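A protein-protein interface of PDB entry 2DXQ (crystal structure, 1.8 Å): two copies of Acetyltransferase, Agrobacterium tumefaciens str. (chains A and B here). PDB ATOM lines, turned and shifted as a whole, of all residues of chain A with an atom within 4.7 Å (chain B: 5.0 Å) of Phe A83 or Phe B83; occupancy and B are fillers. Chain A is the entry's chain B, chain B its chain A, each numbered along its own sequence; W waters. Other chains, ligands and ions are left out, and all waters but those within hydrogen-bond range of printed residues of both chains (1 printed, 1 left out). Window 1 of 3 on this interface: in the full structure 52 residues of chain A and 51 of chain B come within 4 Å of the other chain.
OE2 of Glu A85 sits close to SD of Met B119, 3.6 Å away.
O of Ala B82 lies within hydrogen-bond range of N of Met B119, 2.8 Å away. N of Ile B84 is in hydrogen-bond range of O of Met B119, at 2.9 Å. The backbone NH (N) of Thr A67 is in hydrogen-bond range of the backbone carbonyl oxygen (O) of Glu A85. O of Thr B67 lies within hydrogen-bond range of N of Glu B85 (2.8 Å). The backbone NH (N) of Val A71 lies within hydrogen-bond range of the backbone carbonyl oxygen (O) of Tyr A81 (2.8 Å). The backbone NH (N) of Val B71 sits at hydrogen-bond distance from the backbone carbonyl oxygen (O) of Tyr B81, at 2.8 Å.
OH of Tyr B81 touches CD1 of Leu A69 (3.8 Å). Leu A69 touches Phe B83. CG1 of Val A71 touches CD2 of Leu B69, 3.7 Å away. CD1 of Leu B69 touches CE2 of Phe A83, 3.8 Å away. CD1 of Phe A83 touches CE1 of Phe B83 (3.5 Å). Phe A83 touches Glu B85. CB of Glu A85 touches OH of Tyr B81 (3.4 Å). OE2 of Glu A85 touches CZ of Phe B83, at 3.99 Å. Leu A121 touches Phe B83. CB of Met B119 touches CD2 of Leu A121 (3.8 Å).
Printed residues of chain B within 4 Å of Met A119: Glu B85. Of the printed residues of chain A, Glu B85 touches Tyr A81, Phe A83 and Met A119. The nearest printed residue of chain A that does not touch Phe B83 is Ile A84 (5.6 Å). The nearest printed residue of chain B that does not touch Tyr A81 is Thr B67 (5.1 Å).
Of the 11 printed residues of chain A, 7 touch a printed residue of chain B. Hydrophobic or aromatic side chains of chain A within 4 Å of the printed part of chain B: Leu A69, Val A71, Tyr A81, Phe A83, Met A119 and Leu A121. Along chain A the printed residues that touch a printed residue of chain B span positions 69 to 121. Of the 11 printed residues of chain B, 6 touch a printed residue of chain A. Hydrophobic or aromatic side chains of chain B that line the printed part of chain A: Leu B69, Val B71, Tyr B81, Phe B83 and Met B119. Among the printed residues, no Asp or Glu carboxylate lies within 4 Å of a Lys or Arg side-chain nitrogen of the other chain.
Leu A69 touches Val B71, and with the chains exchanged Val A71 touches Leu B69. Leu A69 touches Tyr B81, and with the chains exchanged Tyr A81 touches Leu B69. Tyr A81 touches Glu B85, and with the chains exchanged Glu A85 touches Tyr B81. Glu A85 touches Met B119, and with the chains exchanged Met A119 touches Glu B85. 10 positions are printed for both chains. Of the 15 pairs that touch across the chains among the printed residues, 13 have their exchanged pair printed and touching as well.
Water W1 lies within hydrogen-bond range of OE2 of Glu B85 and SD of Met A119.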
ATOM      1  N   THR A  67     -12.682  14.728  27.956  1.00  0.00           N
ATOM      2  CA  THR A  67     -12.984  15.404  29.234  1.00  0.00           C
ATOM      3  C   THR A  67     -14.407  15.087  29.674  1.00  0.00           C
ATOM      4  O   THR A  67     -15.341  15.196  28.878  1.00  0.00           O
ATOM      5  CB  THR A  67     -12.765  16.930  29.120  1.00  0.00           C
ATOM      6  OG1 THR A  67     -11.381  17.197  28.840  1.00  0.00           O
ATOM      7  CG2 THR A  67     -13.188  17.667  30.412  1.00  0.00           C
ATOM      8  N   LEU A  68     -14.561  14.660  30.927  1.00  0.00           N
ATOM      9  CA  LEU A  68     -15.874  14.382  31.488  1.00  0.00           C
ATOM     10  C   LEU A  68     -16.273  15.510  32.424  1.00  0.00           C
ATOM     11  O   LEU A  68     -15.476  15.923  33.273  1.00  0.00           O
ATOM     12  CB  LEU A  68     -15.880  13.062  32.263  1.00  0.00           C
ATOM     13  CG  LEU A  68     -17.213  12.636  32.911  1.00  0.00           C
ATOM     14  CD1 LEU A  68     -18.318  12.357  31.866  1.00  0.00           C
ATOM     15  CD2 LEU A  68     -17.035  11.438  33.849  1.00  0.00           C
ATOM     16  N   LEU A  69     -17.502  16.007  32.255  1.00  0.00           N
ATOM     17  CA  LEU A  69     -18.077  17.001  33.183  1.00  0.00           C
ATOM     18  C   LEU A  69     -19.314  16.406  33.844  1.00  0.00           C
ATOM     19  O   LEU A  69     -20.316  16.183  33.191  1.00  0.00           O
ATOM     20  CB  LEU A  69     -18.517  18.263  32.418  1.00  0.00           C
ATOM     21  CG  LEU A  69     -17.480  18.888  31.508  1.00  0.00           C
ATOM     22  CD1 LEU A  69     -18.106  20.020  30.712  1.00  0.00           C
ATOM     23  CD2 LEU A  69     -16.321  19.376  32.353  1.00  0.00           C
ATOM     24  N   VAL A  71     -22.323  17.043  36.413  1.00  0.00           N
ATOM     25  CA  VAL A  71     -23.003  18.267  36.838  1.00  0.00           C
ATOM     26  C   VAL A  71     -24.101  17.964  37.869  1.00  0.00           C
ATOM     27  O   VAL A  71     -24.963  17.122  37.627  1.00  0.00           O
ATOM     28  CB  VAL A  71     -23.650  18.940  35.607  1.00  0.00           C
ATOM     29  CG1 VAL A  71     -24.194  20.342  35.959  1.00  0.00           C
ATOM     30  CG2 VAL A  71     -22.654  18.998  34.397  1.00  0.00           C
ATOM     31  N   TYR A  81     -26.102  14.682  35.769  1.00  0.00           N
ATOM     32  CA  TYR A  81     -25.931  14.339  34.356  1.00  0.00           C
ATOM     33  C   TYR A  81     -24.520  14.740  33.960  1.00  0.00           C
ATOM     34  O   TYR A  81     -23.805  15.425  34.725  1.00  0.00           O
ATOM     35  CB  TYR A  81     -26.995  15.028  33.460  1.00  0.00           C
ATOM     36  CG  TYR A  81     -27.009  16.537  33.561  1.00  0.00           C
ATOM     37  CD1 TYR A  81     -27.855  17.179  34.465  1.00  0.00           C
ATOM     38  CD2 TYR A  81     -26.184  17.327  32.758  1.00  0.00           C
ATOM     39  CE1 TYR A  81     -27.866  18.570  34.589  1.00  0.00           C
ATOM     40  CE2 TYR A  81     -26.185  18.725  32.878  1.00  0.00           C
ATOM     41  CZ  TYR A  81     -27.038  19.334  33.790  1.00  0.00           C
ATOM     42  OH  TYR A  81     -27.048  20.703  33.912  1.00  0.00           O
ATOM     43  N   ALA A  82     -24.095  14.323  32.767  1.00  0.00           N
ATOM     44  CA  ALA A  82     -22.719  14.582  32.369  1.00  0.00           C
ATOM     45  C   ALA A  82     -22.607  15.035  30.931  1.00  0.00           C
ATOM     46  O   ALA A  82     -23.481  14.723  30.122  1.00  0.00           O
ATOM     47  CB  ALA A  82     -21.849  13.310  32.598  1.00  0.00           C
ATOM     48  N   PHE A  83     -21.537  15.768  30.629  1.00  0.00           N
ATOM     49  CA  PHE A  83     -21.153  16.084  29.241  1.00  0.00           C
ATOM     50  C   PHE A  83     -19.773  15.506  28.986  1.00  0.00           C
ATOM     51  O   PHE A  83     -18.974  15.379  29.921  1.00  0.00           O
ATOM     52  CB  PHE A  83     -21.063  17.585  29.011  1.00  0.00           C
ATOM     53  CG  PHE A  83     -22.376  18.300  29.079  1.00  0.00           C
ATOM     54  CD1 PHE A  83     -23.215  18.339  27.965  1.00  0.00           C
ATOM     55  CD2 PHE A  83     -22.755  18.973  30.236  1.00  0.00           C
ATOM     56  CE1 PHE A  83     -24.441  19.021  28.021  1.00  0.00           C
ATOM     57  CE2 PHE A  83     -23.980  19.655  30.294  1.00  0.00           C
ATOM     58  CZ  PHE A  83     -24.808  19.683  29.184  1.00  0.00           C
ATOM     59  N   ILE A  84     -19.494  15.174  27.724  1.00  0.00           N
ATOM     60  CA  ILE A  84     -18.139  14.805  27.317  1.00  0.00           C
ATOM     61  C   ILE A  84     -17.683  15.816  26.289  1.00  0.00           C
ATOM     62  O   ILE A  84     -18.435  16.177  25.363  1.00  0.00           O
ATOM     63  CB  ILE A  84     -18.054  13.356  26.787  1.00  0.00           C
ATOM     64  CG1 ILE A  84     -18.202  12.380  27.964  1.00  0.00           C
ATOM     65  CG2 ILE A  84     -16.693  13.118  26.060  1.00  0.00           C
ATOM     66  CD1 ILE A  84     -18.396  10.954  27.562  1.00  0.00           C
ATOM     67  N   GLU A  85     -16.455  16.289  26.452  1.00  0.00           N
ATOM     68  CA  GLU A  85     -15.896  17.295  25.572  1.00  0.00           C
ATOM     69  C   GLU A  85     -14.457  16.994  25.177  1.00  0.00           C
ATOM     70  O   GLU A  85     -13.789  16.192  25.821  1.00  0.00           O
ATOM     71  CB  GLU A  85     -15.949  18.677  26.222  1.00  0.00           C
ATOM     72  CG  GLU A  85     -17.199  19.489  25.882  1.00  0.00           C
ATOM     73  CD  GLU A  85     -17.289  19.846  24.396  1.00  0.00           C
ATOM     74  OE1 GLU A  85     -16.265  19.760  23.681  1.00  0.00           O
ATOM     75  OE2 GLU A  85     -18.389  20.207  23.939  1.00  0.00           O
ATOM     76  N   MET A 119     -24.155  13.338  27.712  1.00  0.00           N
ATOM     77  CA  MET A 119     -24.423  14.031  26.447  1.00  0.00           C
ATOM     78  C   MET A 119     -23.156  14.557  25.811  1.00  0.00           C
ATOM     79  O   MET A 119     -22.160  14.812  26.482  1.00  0.00           O
ATOM     80  CB  MET A 119     -25.391  15.203  26.668  1.00  0.00           C
ATOM     81  CG  MET A 119     -26.707  14.796  27.232  1.00  0.00           C
ATOM     82  SD  MET A 119     -27.768  16.372  27.627  1.00  0.00           S
ATOM     83  CE  MET A 119     -26.868  16.921  29.251  1.00  0.00           C
ATOM     84  N   LEU A 121     -21.997  17.207  22.187  1.00  0.00           N
ATOM     85  CA  LEU A 121     -22.314  17.938  20.962  1.00  0.00           C
ATOM     86  C   LEU A 121     -21.140  17.832  20.023  1.00  0.00           C
ATOM     87  O   LEU A 121     -19.965  17.970  20.429  1.00  0.00           O
ATOM     88  CB  LEU A 121     -22.589  19.425  21.244  1.00  0.00           C
ATOM     89  CG  LEU A 121     -23.834  19.764  22.066  1.00  0.00           C
ATOM     90  CD1 LEU A 121     -23.534  19.783  23.569  1.00  0.00           C
ATOM     91  CD2 LEU A 121     -24.402  21.120  21.635  1.00  0.00           C
ATOM     92  N   THR B  67     -30.134  27.269  33.646  1.00  0.00           N
ATOM     93  CA  THR B  67     -28.895  27.076  34.391  1.00  0.00           C
ATOM     94  C   THR B  67     -27.714  27.229  33.440  1.00  0.00           C
ATOM     95  O   THR B  67     -27.681  26.611  32.372  1.00  0.00           O
ATOM     96  CB  THR B  67     -28.866  25.686  35.047  1.00  0.00           C
ATOM     97  OG1 THR B  67     -29.991  25.552  35.937  1.00  0.00           O
ATOM     98  CG2 THR B  67     -27.526  25.447  35.797  1.00  0.00           C
ATOM     99  N   LEU B  68     -26.753  28.053  33.846  1.00  0.00           N
ATOM    100  CA  LEU B  68     -25.550  28.286  33.068  1.00  0.00           C
ATOM    101  C   LEU B  68     -24.403  27.505  33.682  1.00  0.00           C
ATOM    102  O   LEU B  68     -24.192  27.561  34.893  1.00  0.00           O
ATOM    103  CB  LEU B  68     -25.203  29.775  33.065  1.00  0.00           C
ATOM    104  CG  LEU B  68     -23.920  30.191  32.354  1.00  0.00           C
ATOM    105  CD1 LEU B  68     -23.972  29.864  30.846  1.00  0.00           C
ATOM    106  CD2 LEU B  68     -23.721  31.698  32.596  1.00  0.00           C
ATOM    107  N   LEU B  69     -23.656  26.802  32.833  1.00  0.00           N
ATOM    108  CA  LEU B  69     -22.482  26.047  33.279  1.00  0.00           C
ATOM    109  C   LEU B  69     -21.281  26.578  32.507  1.00  0.00           C
ATOM    110  O   LEU B  69     -21.177  26.384  31.299  1.00  0.00           O
ATOM    111  CB  LEU B  69     -22.660  24.548  33.001  1.00  0.00           C
ATOM    112  CG  LEU B  69     -23.999  23.910  33.400  1.00  0.00           C
ATOM    113  CD1 LEU B  69     -24.110  22.503  32.827  1.00  0.00           C
ATOM    114  CD2 LEU B  69     -24.132  23.888  34.928  1.00  0.00           C
ATOM    115  N   VAL B  71     -17.261  26.475  31.904  1.00  0.00           N
ATOM    116  CA  VAL B  71     -16.284  25.379  32.038  1.00  0.00           C
ATOM    117  C   VAL B  71     -14.884  25.869  31.659  1.00  0.00           C
ATOM    118  O   VAL B  71     -14.704  26.413  30.574  1.00  0.00           O
ATOM    119  CB  VAL B  71     -16.658  24.195  31.105  1.00  0.00           C
ATOM    120  CG1 VAL B  71     -15.778  22.965  31.418  1.00  0.00           C
ATOM    121  CG2 VAL B  71     -18.154  23.826  31.222  1.00  0.00           C
ATOM    122  N   TYR B  81     -15.831  27.567  27.817  1.00  0.00           N
ATOM    123  CA  TYR B  81     -17.050  27.439  27.031  1.00  0.00           C
ATOM    124  C   TYR B  81     -18.183  27.185  28.009  1.00  0.00           C
ATOM    125  O   TYR B  81     -17.955  26.915  29.199  1.00  0.00           O
ATOM    126  CB  TYR B  81     -16.953  26.318  25.976  1.00  0.00           C
ATOM    127  CG  TYR B  81     -16.561  24.995  26.574  1.00  0.00           C
ATOM    128  CD1 TYR B  81     -15.221  24.604  26.611  1.00  0.00           C
ATOM    129  CD2 TYR B  81     -17.522  24.134  27.097  1.00  0.00           C
ATOM    130  CE1 TYR B  81     -14.845  23.395  27.184  1.00  0.00           C
ATOM    131  CE2 TYR B  81     -17.159  22.923  27.684  1.00  0.00           C
ATOM    132  CZ  TYR B  81     -15.817  22.560  27.718  1.00  0.00           C
ATOM    133  OH  TYR B  81     -15.460  21.356  28.269  1.00  0.00           O
ATOM    134  N   ALA B  82     -19.414  27.240  27.520  1.00  0.00           N
ATOM    135  CA  ALA B  82     -20.539  27.109  28.430  1.00  0.00           C
ATOM    136  C   ALA B  82     -21.630  26.240  27.849  1.00  0.00           C
ATOM    137  O   ALA B  82     -21.755  26.131  26.625  1.00  0.00           O
ATOM    138  CB  ALA B  82     -21.103  28.486  28.765  1.00  0.00           C
ATOM    139  N   PHE B  83     -22.413  25.633  28.739  1.00  0.00           N
ATOM    140  CA  PHE B  83     -23.676  24.993  28.370  1.00  0.00           C
ATOM    141  C   PHE B  83     -24.810  25.702  29.085  1.00  0.00           C
ATOM    142  O   PHE B  83     -24.629  26.256  30.190  1.00  0.00           O
ATOM    143  CB  PHE B  83     -23.712  23.551  28.852  1.00  0.00           C
ATOM    144  CG  PHE B  83     -22.703  22.658  28.196  1.00  0.00           C
ATOM    145  CD1 PHE B  83     -22.996  22.035  26.995  1.00  0.00           C
ATOM    146  CD2 PHE B  83     -21.477  22.428  28.800  1.00  0.00           C
ATOM    147  CE1 PHE B  83     -22.062  21.197  26.384  1.00  0.00           C
ATOM    148  CE2 PHE B  83     -20.539  21.577  28.208  1.00  0.00           C
ATOM    149  CZ  PHE B  83     -20.836  20.960  26.999  1.00  0.00           C
ATOM    150  N   ILE B  84     -25.991  25.635  28.490  1.00  0.00           N
ATOM    151  CA  ILE B  84     -27.213  26.060  29.187  1.00  0.00           C
ATOM    152  C   ILE B  84     -28.152  24.871  29.328  1.00  0.00           C
ATOM    153  O   ILE B  84     -28.385  24.137  28.353  1.00  0.00           O
ATOM    154  CB  ILE B  84     -27.887  27.259  28.483  1.00  0.00           C
ATOM    155  CG1 ILE B  84     -27.006  28.508  28.658  1.00  0.00           C
ATOM    156  CG2 ILE B  84     -29.291  27.524  29.065  1.00  0.00           C
ATOM    157  CD1 ILE B  84     -27.514  29.723  27.894  1.00  0.00           C
ATOM    158  N   GLU B  85     -28.658  24.664  30.542  1.00  0.00           N
ATOM    159  CA  GLU B  85     -29.468  23.488  30.843  1.00  0.00           C
ATOM    160  C   GLU B  85     -30.719  23.827  31.639  1.00  0.00           C
ATOM    161  O   GLU B  85     -30.845  24.916  32.189  1.00  0.00           O
ATOM    162  CB  GLU B  85     -28.637  22.464  31.631  1.00  0.00           C
ATOM    163  CG  GLU B  85     -27.946  21.418  30.726  1.00  0.00           C
ATOM    164  CD  GLU B  85     -28.950  20.535  30.010  1.00  0.00           C
ATOM    165  OE1 GLU B  85     -30.149  20.564  30.384  1.00  0.00           O
ATOM    166  OE2 GLU B  85     -28.560  19.829  29.053  1.00  0.00           O
ATOM    167  N   VAL B 118     -21.434  29.106  23.506  1.00  0.00           N
ATOM    168  CA  VAL B 118     -22.424  28.600  24.449  1.00  0.00           C
ATOM    169  C   VAL B 118     -23.219  27.517  23.719  1.00  0.00           C
ATOM    170  O   VAL B 118     -23.687  27.754  22.617  1.00  0.00           O
ATOM    171  CB  VAL B 118     -23.368  29.725  24.947  1.00  0.00           C
ATOM    172  CG1 VAL B 118     -24.369  29.165  25.970  1.00  0.00           C
ATOM    173  CG2 VAL B 118     -22.552  30.849  25.588  1.00  0.00           C
ATOM    174  N   MET B 119     -23.382  26.354  24.349  1.00  0.00           N
ATOM    175  CA  MET B 119     -24.061  25.220  23.713  1.00  0.00           C
ATOM    176  C   MET B 119     -25.323  24.825  24.469  1.00  0.00           C
ATOM    177  O   MET B 119     -25.432  25.039  25.676  1.00  0.00           O
ATOM    178  CB  MET B 119     -23.111  24.018  23.656  1.00  0.00           C
ATOM    179  CG  MET B 119     -21.944  24.239  22.713  1.00  0.00           C
ATOM    180  SD  MET B 119     -20.617  22.822  22.958  1.00  0.00           S
ATOM    181  CE  MET B 119     -19.925  23.406  24.653  1.00  0.00           C
HETATM  182  O   HOH W   1     -30.455  18.594  27.683  1.00  0.00           O
